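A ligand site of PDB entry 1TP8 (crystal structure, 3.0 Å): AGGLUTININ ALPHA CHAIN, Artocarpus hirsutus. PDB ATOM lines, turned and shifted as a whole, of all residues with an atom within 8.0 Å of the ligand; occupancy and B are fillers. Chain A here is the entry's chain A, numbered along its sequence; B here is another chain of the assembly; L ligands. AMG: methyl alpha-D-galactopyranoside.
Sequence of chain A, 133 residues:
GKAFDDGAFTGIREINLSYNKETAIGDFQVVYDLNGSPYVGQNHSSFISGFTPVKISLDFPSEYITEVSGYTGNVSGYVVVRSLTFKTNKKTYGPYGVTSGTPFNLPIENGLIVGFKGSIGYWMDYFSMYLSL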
ATOM      1  N   GLY A   1       3.774  16.380  32.590  1.00  0.00           N
ATOM      2  CA  GLY A   1       4.798  15.684  31.784  1.00  0.00           C
ATOM      3  C   GLY A   1       5.903  16.648  31.339  1.00  0.00           C
ATOM      4  O   GLY A   1       5.839  17.842  31.644  1.00  0.00           O
ATOM      5  N   LYS A   2       6.911  16.160  30.637  1.00  0.00           N
ATOM      6  CA  LYS A   2       7.996  17.041  30.211  1.00  0.00           C
ATOM      7  C   LYS A   2       7.807  17.512  28.787  1.00  0.00           C
ATOM      8  O   LYS A   2       7.902  16.711  27.853  1.00  0.00           O
ATOM      9  CB  LYS A   2       9.318  16.293  30.382  1.00  0.00           C
ATOM     10  CG  LYS A   2      10.563  17.022  29.927  1.00  0.00           C
ATOM     11  CD  LYS A   2      10.835  18.215  30.838  1.00  0.00           C
ATOM     12  CE  LYS A   2      12.040  18.994  30.352  1.00  0.00           C
ATOM     13  NZ  LYS A   2      13.206  18.089  30.061  1.00  0.00           N
ATOM     14  N   ALA A  24      -0.939   3.255  26.738  1.00  0.00           N
ATOM     15  CA  ALA A  24      -0.880   4.308  25.727  1.00  0.00           C
ATOM     16  C   ALA A  24       0.459   4.399  25.013  1.00  0.00           C
ATOM     17  O   ALA A  24       1.132   3.375  24.810  1.00  0.00           O
ATOM     18  CB  ALA A  24      -1.188   5.615  26.465  1.00  0.00           C
ATOM     19  N   ILE A  25       0.886   5.581  24.570  1.00  0.00           N
ATOM     20  CA  ILE A  25       2.148   5.749  23.867  1.00  0.00           C
ATOM     21  C   ILE A  25       3.194   6.281  24.842  1.00  0.00           C
ATOM     22  O   ILE A  25       2.865   7.163  25.640  1.00  0.00           O
ATOM     23  CB  ILE A  25       1.983   6.720  22.696  1.00  0.00           C
ATOM     24  CG1 ILE A  25       0.861   6.253  21.767  1.00  0.00           C
ATOM     25  CG2 ILE A  25       3.262   6.951  21.905  1.00  0.00           C
ATOM     26  CD1 ILE A  25       1.116   5.248  20.694  1.00  0.00           C
ATOM     27  N   SER A  46       9.816   8.309  28.225  1.00  0.00           N
ATOM     28  CA  SER A  46       8.786   8.259  29.250  1.00  0.00           C
ATOM     29  C   SER A  46       9.414   8.095  30.635  1.00  0.00           C
ATOM     30  O   SER A  46      10.496   7.541  30.837  1.00  0.00           O
ATOM     31  CB  SER A  46       7.873   7.077  28.982  1.00  0.00           C
ATOM     32  OG  SER A  46       7.262   6.543  30.142  1.00  0.00           O
ATOM     33  N   PHE A  47       8.704   8.545  31.650  1.00  0.00           N
ATOM     34  CA  PHE A  47       9.118   8.438  33.031  1.00  0.00           C
ATOM     35  C   PHE A  47       9.098   7.012  33.525  1.00  0.00           C
ATOM     36  O   PHE A  47       9.569   6.863  34.666  1.00  0.00           O
ATOM     37  CB  PHE A  47       8.167   9.207  33.942  1.00  0.00           C
ATOM     38  CG  PHE A  47       8.156  10.707  33.799  1.00  0.00           C
ATOM     39  CD1 PHE A  47       8.977  11.331  32.878  1.00  0.00           C
ATOM     40  CD2 PHE A  47       7.309  11.491  34.562  1.00  0.00           C
ATOM     41  CE1 PHE A  47       8.979  12.697  32.731  1.00  0.00           C
ATOM     42  CE2 PHE A  47       7.304  12.864  34.412  1.00  0.00           C
ATOM     43  CZ  PHE A  47       8.134  13.459  33.503  1.00  0.00           C
ATOM     44  N   ILE A  48       8.455   6.041  32.881  1.00  0.00           N
ATOM     45  CA  ILE A  48       8.429   4.675  33.395  1.00  0.00           C
ATOM     46  C   ILE A  48       8.897   3.690  32.339  1.00  0.00           C
ATOM     47  O   ILE A  48       9.323   4.147  31.294  1.00  0.00           O
ATOM     48  CB  ILE A  48       7.057   4.287  33.940  1.00  0.00           C
ATOM     49  CG1 ILE A  48       6.028   4.220  32.810  1.00  0.00           C
ATOM     50  CG2 ILE A  48       6.593   5.233  35.028  1.00  0.00           C
ATOM     51  CD1 ILE A  48       4.743   3.541  33.235  1.00  0.00           C
ATOM     52  N   VAL A  75      -6.382   7.869  30.821  1.00  0.00           N
ATOM     53  CA  VAL A  75      -5.652   6.773  31.448  1.00  0.00           C
ATOM     54  C   VAL A  75      -5.230   7.269  32.832  1.00  0.00           C
ATOM     55  O   VAL A  75      -4.630   8.330  32.969  1.00  0.00           O
ATOM     56  CB  VAL A  75      -4.416   6.274  30.730  1.00  0.00           C
ATOM     57  CG1 VAL A  75      -3.682   5.300  31.644  1.00  0.00           C
ATOM     58  CG2 VAL A  75      -4.758   5.612  29.419  1.00  0.00           C
ATOM     59  N   SER A  76      -5.628   6.530  33.866  1.00  0.00           N
ATOM     60  CA  SER A  76      -5.381   6.864  35.256  1.00  0.00           C
ATOM     61  C   SER A  76      -5.743   8.309  35.550  1.00  0.00           C
ATOM     62  O   SER A  76      -4.997   9.008  36.212  1.00  0.00           O
ATOM     63  CB  SER A  76      -3.940   6.544  35.645  1.00  0.00           C
ATOM     64  OG  SER A  76      -3.697   6.633  37.045  1.00  0.00           O
ATOM     65  N   GLY A  77      -6.895   8.810  35.091  1.00  0.00           N
ATOM     66  CA  GLY A  77      -7.338  10.150  35.295  1.00  0.00           C
ATOM     67  C   GLY A  77      -6.671  11.262  34.524  1.00  0.00           C
ATOM     68  O   GLY A  77      -6.900  12.441  34.759  1.00  0.00           O
ATOM     69  N   TYR A  78      -5.778  10.955  33.603  1.00  0.00           N
ATOM     70  CA  TYR A  78      -5.027  11.866  32.790  1.00  0.00           C
ATOM     71  C   TYR A  78      -5.451  11.796  31.328  1.00  0.00           C
ATOM     72  O   TYR A  78      -5.850  10.703  30.930  1.00  0.00           O
ATOM     73  CB  TYR A  78      -3.557  11.449  32.845  1.00  0.00           C
ATOM     74  CG  TYR A  78      -2.876  11.736  34.159  1.00  0.00           C
ATOM     75  CD1 TYR A  78      -2.490  13.025  34.475  1.00  0.00           C
ATOM     76  CD2 TYR A  78      -2.606  10.710  35.058  1.00  0.00           C
ATOM     77  CE1 TYR A  78      -1.843  13.310  35.665  1.00  0.00           C
ATOM     78  CE2 TYR A  78      -1.965  10.994  36.257  1.00  0.00           C
ATOM     79  CZ  TYR A  78      -1.592  12.290  36.553  1.00  0.00           C
ATOM     80  OH  TYR A  78      -0.952  12.530  37.755  1.00  0.00           O
ATOM     81  N   VAL A  79      -5.358  12.903  30.587  1.00  0.00           N
ATOM     82  CA  VAL A  79      -5.664  12.755  29.156  1.00  0.00           C
ATOM     83  C   VAL A  79      -4.366  12.558  28.368  1.00  0.00           C
ATOM     84  O   VAL A  79      -3.460  13.355  28.506  1.00  0.00           O
ATOM     85  CB  VAL A  79      -6.466  13.877  28.545  1.00  0.00           C
ATOM     86  CG1 VAL A  79      -6.849  13.504  27.127  1.00  0.00           C
ATOM     87  CG2 VAL A  79      -7.698  14.098  29.372  1.00  0.00           C
ATOM     88  N   VAL A  80      -4.272  11.472  27.636  1.00  0.00           N
ATOM     89  CA  VAL A  80      -3.067  11.053  26.937  1.00  0.00           C
ATOM     90  C   VAL A  80      -3.373  10.557  25.535  1.00  0.00           C
ATOM     91  O   VAL A  80      -4.544  10.261  25.238  1.00  0.00           O
ATOM     92  CB  VAL A  80      -2.416   9.874  27.702  1.00  0.00           C
ATOM     93  CG1 VAL A  80      -1.946  10.236  29.106  1.00  0.00           C
ATOM     94  CG2 VAL A  80      -3.346   8.677  27.815  1.00  0.00           C
ATOM     95  N   VAL A  81      -2.319  10.427  24.701  1.00  0.00           N
ATOM     96  CA  VAL A  81      -2.508   9.919  23.318  1.00  0.00           C
ATOM     97  C   VAL A  81      -2.476   8.399  23.346  1.00  0.00           C
ATOM     98  O   VAL A  81      -1.432   7.816  23.689  1.00  0.00           O
ATOM     99  CB  VAL A  81      -1.439  10.511  22.390  1.00  0.00           C
ATOM    100  CG1 VAL A  81      -1.610  10.107  20.941  1.00  0.00           C
ATOM    101  CG2 VAL A  81      -1.459  12.029  22.493  1.00  0.00           C
ATOM    102  N   SER A 119       4.501  16.617  24.612  1.00  0.00           N
ATOM    103  CA  SER A 119       4.828  16.455  26.021  1.00  0.00           C
ATOM    104  C   SER A 119       4.628  15.030  26.475  1.00  0.00           C
ATOM    105  O   SER A 119       3.654  14.398  26.051  1.00  0.00           O
ATOM    106  CB  SER A 119       3.951  17.414  26.847  1.00  0.00           C
ATOM    107  OG  SER A 119       4.278  17.187  28.206  1.00  0.00           O
ATOM    108  N   ILE A 120       5.545  14.490  27.270  1.00  0.00           N
ATOM    109  CA  ILE A 120       5.460  13.135  27.769  1.00  0.00           C
ATOM    110  C   ILE A 120       5.709  13.104  29.273  1.00  0.00           C
ATOM    111  O   ILE A 120       6.616  13.757  29.754  1.00  0.00           O
ATOM    112  CB  ILE A 120       6.501  12.146  27.200  1.00  0.00           C
ATOM    113  CG1 ILE A 120       6.770  12.399  25.719  1.00  0.00           C
ATOM    114  CG2 ILE A 120       6.022  10.737  27.474  1.00  0.00           C
ATOM    115  CD1 ILE A 120       7.096  11.259  24.805  1.00  0.00           C
ATOM    116  N   GLY A 121       4.897  12.330  29.973  1.00  0.00           N
ATOM    117  CA  GLY A 121       5.116  12.136  31.436  1.00  0.00           C
ATOM    118  C   GLY A 121       5.206  10.605  31.541  1.00  0.00           C
ATOM    119  O   GLY A 121       6.163   9.991  31.049  1.00  0.00           O
ATOM    120  N   TYR A 122       4.158   9.996  32.108  1.00  0.00           N
ATOM    121  CA  TYR A 122       4.155   8.534  32.111  1.00  0.00           C
ATOM    122  C   TYR A 122       3.935   8.102  30.671  1.00  0.00           C
ATOM    123  O   TYR A 122       4.623   7.218  30.173  1.00  0.00           O
ATOM    124  CB  TYR A 122       3.057   8.006  33.018  1.00  0.00           C
ATOM    125  CG  TYR A 122       3.541   7.774  34.424  1.00  0.00           C
ATOM    126  CD1 TYR A 122       4.475   8.626  35.000  1.00  0.00           C
ATOM    127  CD2 TYR A 122       3.048   6.717  35.179  1.00  0.00           C
ATOM    128  CE1 TYR A 122       4.899   8.408  36.306  1.00  0.00           C
ATOM    129  CE2 TYR A 122       3.466   6.506  36.482  1.00  0.00           C
ATOM    130  CZ  TYR A 122       4.395   7.354  37.029  1.00  0.00           C
ATOM    131  OH  TYR A 122       4.855   7.187  38.307  1.00  0.00           O
ATOM    132  N   TRP A 123       2.910   8.679  30.055  1.00  0.00           N
ATOM    133  CA  TRP A 123       2.519   8.502  28.671  1.00  0.00           C
ATOM    134  C   TRP A 123       2.591   9.819  27.895  1.00  0.00           C
ATOM    135  O   TRP A 123       2.741  10.906  28.476  1.00  0.00           O
ATOM    136  CB  TRP A 123       1.093   7.917  28.582  1.00  0.00           C
ATOM    137  CG  TRP A 123       0.986   6.761  29.527  1.00  0.00           C
ATOM    138  CD1 TRP A 123       1.474   5.504  29.320  1.00  0.00           C
ATOM    139  CD2 TRP A 123       0.441   6.780  30.843  1.00  0.00           C
ATOM    140  NE1 TRP A 123       1.235   4.735  30.435  1.00  0.00           N
ATOM    141  CE2 TRP A 123       0.605   5.488  31.381  1.00  0.00           C
ATOM    142  CE3 TRP A 123      -0.180   7.747  31.640  1.00  0.00           C
ATOM    143  CZ2 TRP A 123       0.172   5.150  32.668  1.00  0.00           C
ATOM    144  CZ3 TRP A 123      -0.596   7.405  32.913  1.00  0.00           C
ATOM    145  CH2 TRP A 123      -0.433   6.117  33.427  1.00  0.00           C
ATOM    146  N   MET A 124       2.571   9.766  26.559  1.00  0.00           N
ATOM    147  CA  MET A 124       2.573  10.974  25.750  1.00  0.00           C
ATOM    148  C   MET A 124       1.338  11.823  26.031  1.00  0.00           C
ATOM    149  O   MET A 124       0.205  11.377  25.706  1.00  0.00           O
ATOM    150  CB  MET A 124       2.591  10.548  24.280  1.00  0.00           C
ATOM    151  CG  MET A 124       2.569  11.765  23.381  1.00  0.00           C
ATOM    152  SD  MET A 124       2.543  11.491  21.638  1.00  0.00           S
ATOM    153  CE  MET A 124       4.208  11.043  21.194  1.00  0.00           C
ATOM    154  N   ASP A 125       1.455  13.004  26.633  1.00  0.00           N
ATOM    155  CA  ASP A 125       0.302  13.837  26.993  1.00  0.00           C
ATOM    156  C   ASP A 125      -0.456  14.475  25.835  1.00  0.00           C
ATOM    157  O   ASP A 125      -1.683  14.509  25.774  1.00  0.00           O
ATOM    158  CB  ASP A 125       0.772  14.963  27.918  1.00  0.00           C
ATOM    159  CG  ASP A 125       1.522  14.460  29.134  1.00  0.00           C
ATOM    160  OD1 ASP A 125       0.896  13.906  30.058  1.00  0.00           O
ATOM    161  OD2 ASP A 125       2.752  14.631  29.164  1.00  0.00           O
ATOM    162  N   TYR A 126       0.263  15.023  24.865  1.00  0.00           N
ATOM    163  CA  TYR A 126      -0.321  15.605  23.669  1.00  0.00           C
ATOM    164  C   TYR A 126       0.727  15.835  22.593  1.00  0.00           C
ATOM    165  O   TYR A 126       1.887  15.776  22.960  1.00  0.00           O
ATOM    166  CB  TYR A 126      -0.939  16.951  24.023  1.00  0.00           C
ATOM    167  CG  TYR A 126       0.030  17.977  24.560  1.00  0.00           C
ATOM    168  CD1 TYR A 126       0.931  18.669  23.782  1.00  0.00           C
ATOM    169  CD2 TYR A 126      -0.020  18.263  25.918  1.00  0.00           C
ATOM    170  CE1 TYR A 126       1.805  19.597  24.332  1.00  0.00           C
ATOM    171  CE2 TYR A 126       0.825  19.191  26.496  1.00  0.00           C
ATOM    172  CZ  TYR A 126       1.735  19.852  25.694  1.00  0.00           C
ATOM    173  OH  TYR A 126       2.562  20.784  26.286  1.00  0.00           O
ATOM    174  N   ALA B  17      -4.041  16.009  26.018  1.00  0.00           N
ATOM    175  CA  ALA B  17      -4.312  16.890  27.141  1.00  0.00           C
ATOM    176  C   ALA B  17      -4.424  18.347  26.760  1.00  0.00           C
ATOM    177  O   ALA B  17      -3.877  18.761  25.753  1.00  0.00           O
ATOM    178  CB  ALA B  17      -3.176  16.755  28.145  1.00  0.00           C
HETATM  179  C1  AMG L   1       2.711  11.720  35.235  1.00  0.00           C
HETATM  180  C2  AMG L   1       2.883  13.239  35.200  1.00  0.00           C
HETATM  181  C3  AMG L   1       1.573  13.919  34.790  1.00  0.00           C
HETATM  182  C4  AMG L   1       1.012  13.301  33.519  1.00  0.00           C
HETATM  183  C5  AMG L   1       1.002  11.788  33.582  1.00  0.00           C
HETATM  184  C6  AMG L   1       0.573  11.134  32.310  1.00  0.00           C
HETATM  185  C7  AMG L   1       1.456  10.150  36.431  1.00  0.00           C
HETATM  186  O1  AMG L   1       1.684  11.523  36.184  1.00  0.00           O
HETATM  187  O2  AMG L   1       3.299  13.625  36.484  1.00  0.00           O
HETATM  188  O3  AMG L   1       1.863  15.306  34.539  1.00  0.00           O
HETATM  189  O4  AMG L   1       1.862  13.648  32.439  1.00  0.00           O
HETATM  190  O5  AMG L   1       2.338  11.309  33.902  1.00  0.00           O
HETATM  191  O6  AMG L   1       1.485  11.149  31.232  1.00  0.00           O
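OD1 of Asp 125 lies within hydrogen-bond range of O4 of the ligand (2.6 Å). The side-chain hydroxyl of Tyr 78 lies within hydrogen-bond range of an oxygen (O1) of the ligand (3.2 Å). An oxygen (O6) of the ligand is in hydrogen-bond range of the backbone NH (N) of Trp 123 (3.1 Å). The backbone carbonyl oxygen (O) of Trp 123 is in hydrogen-bond range of an oxygen (O6) of the ligand, at 3.0 Å. An oxygen (O3) of the ligand sits at hydrogen-bond distance from the backbone NH of Gly 1 (2.9 Å). The backbone NH of Tyr 122 is in hydrogen-bond range of an oxygen (O5) of the ligand, at 2.9 Å.
O of Tyr 122 sits at hydrogen-bond distance from OG of Ser 46 (2.7 Å). The backbone carbonyl oxygen (O) of Asp 125 lies within hydrogen-bond range of the backbone NH (N) of Ala 17 of chain B (2.8 Å). OD2 of Asp 125 lies within hydrogen-bond range of N of Gly 121. The backbone NH (N) of Asp 125 is in hydrogen-bond range of the backbone carbonyl oxygen (O) of Ser 119 (2.7 Å). The backbone NH (N) of Ile 120 lies close to the side-chain carboxylate (OD2) of Asp 125 (3.4 Å). The backbone carbonyl oxygen (O) of Gly 121 is in hydrogen-bond range of the backbone NH (N) of Phe 47.
Merely in contact with the ligand: Gly 121 (3.7 Å). Of the 23 residues printed, 6 come within 4 Å of the ligand. The nearest printed residue that does not touch the ligand is Val 80 (4.1 Å).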
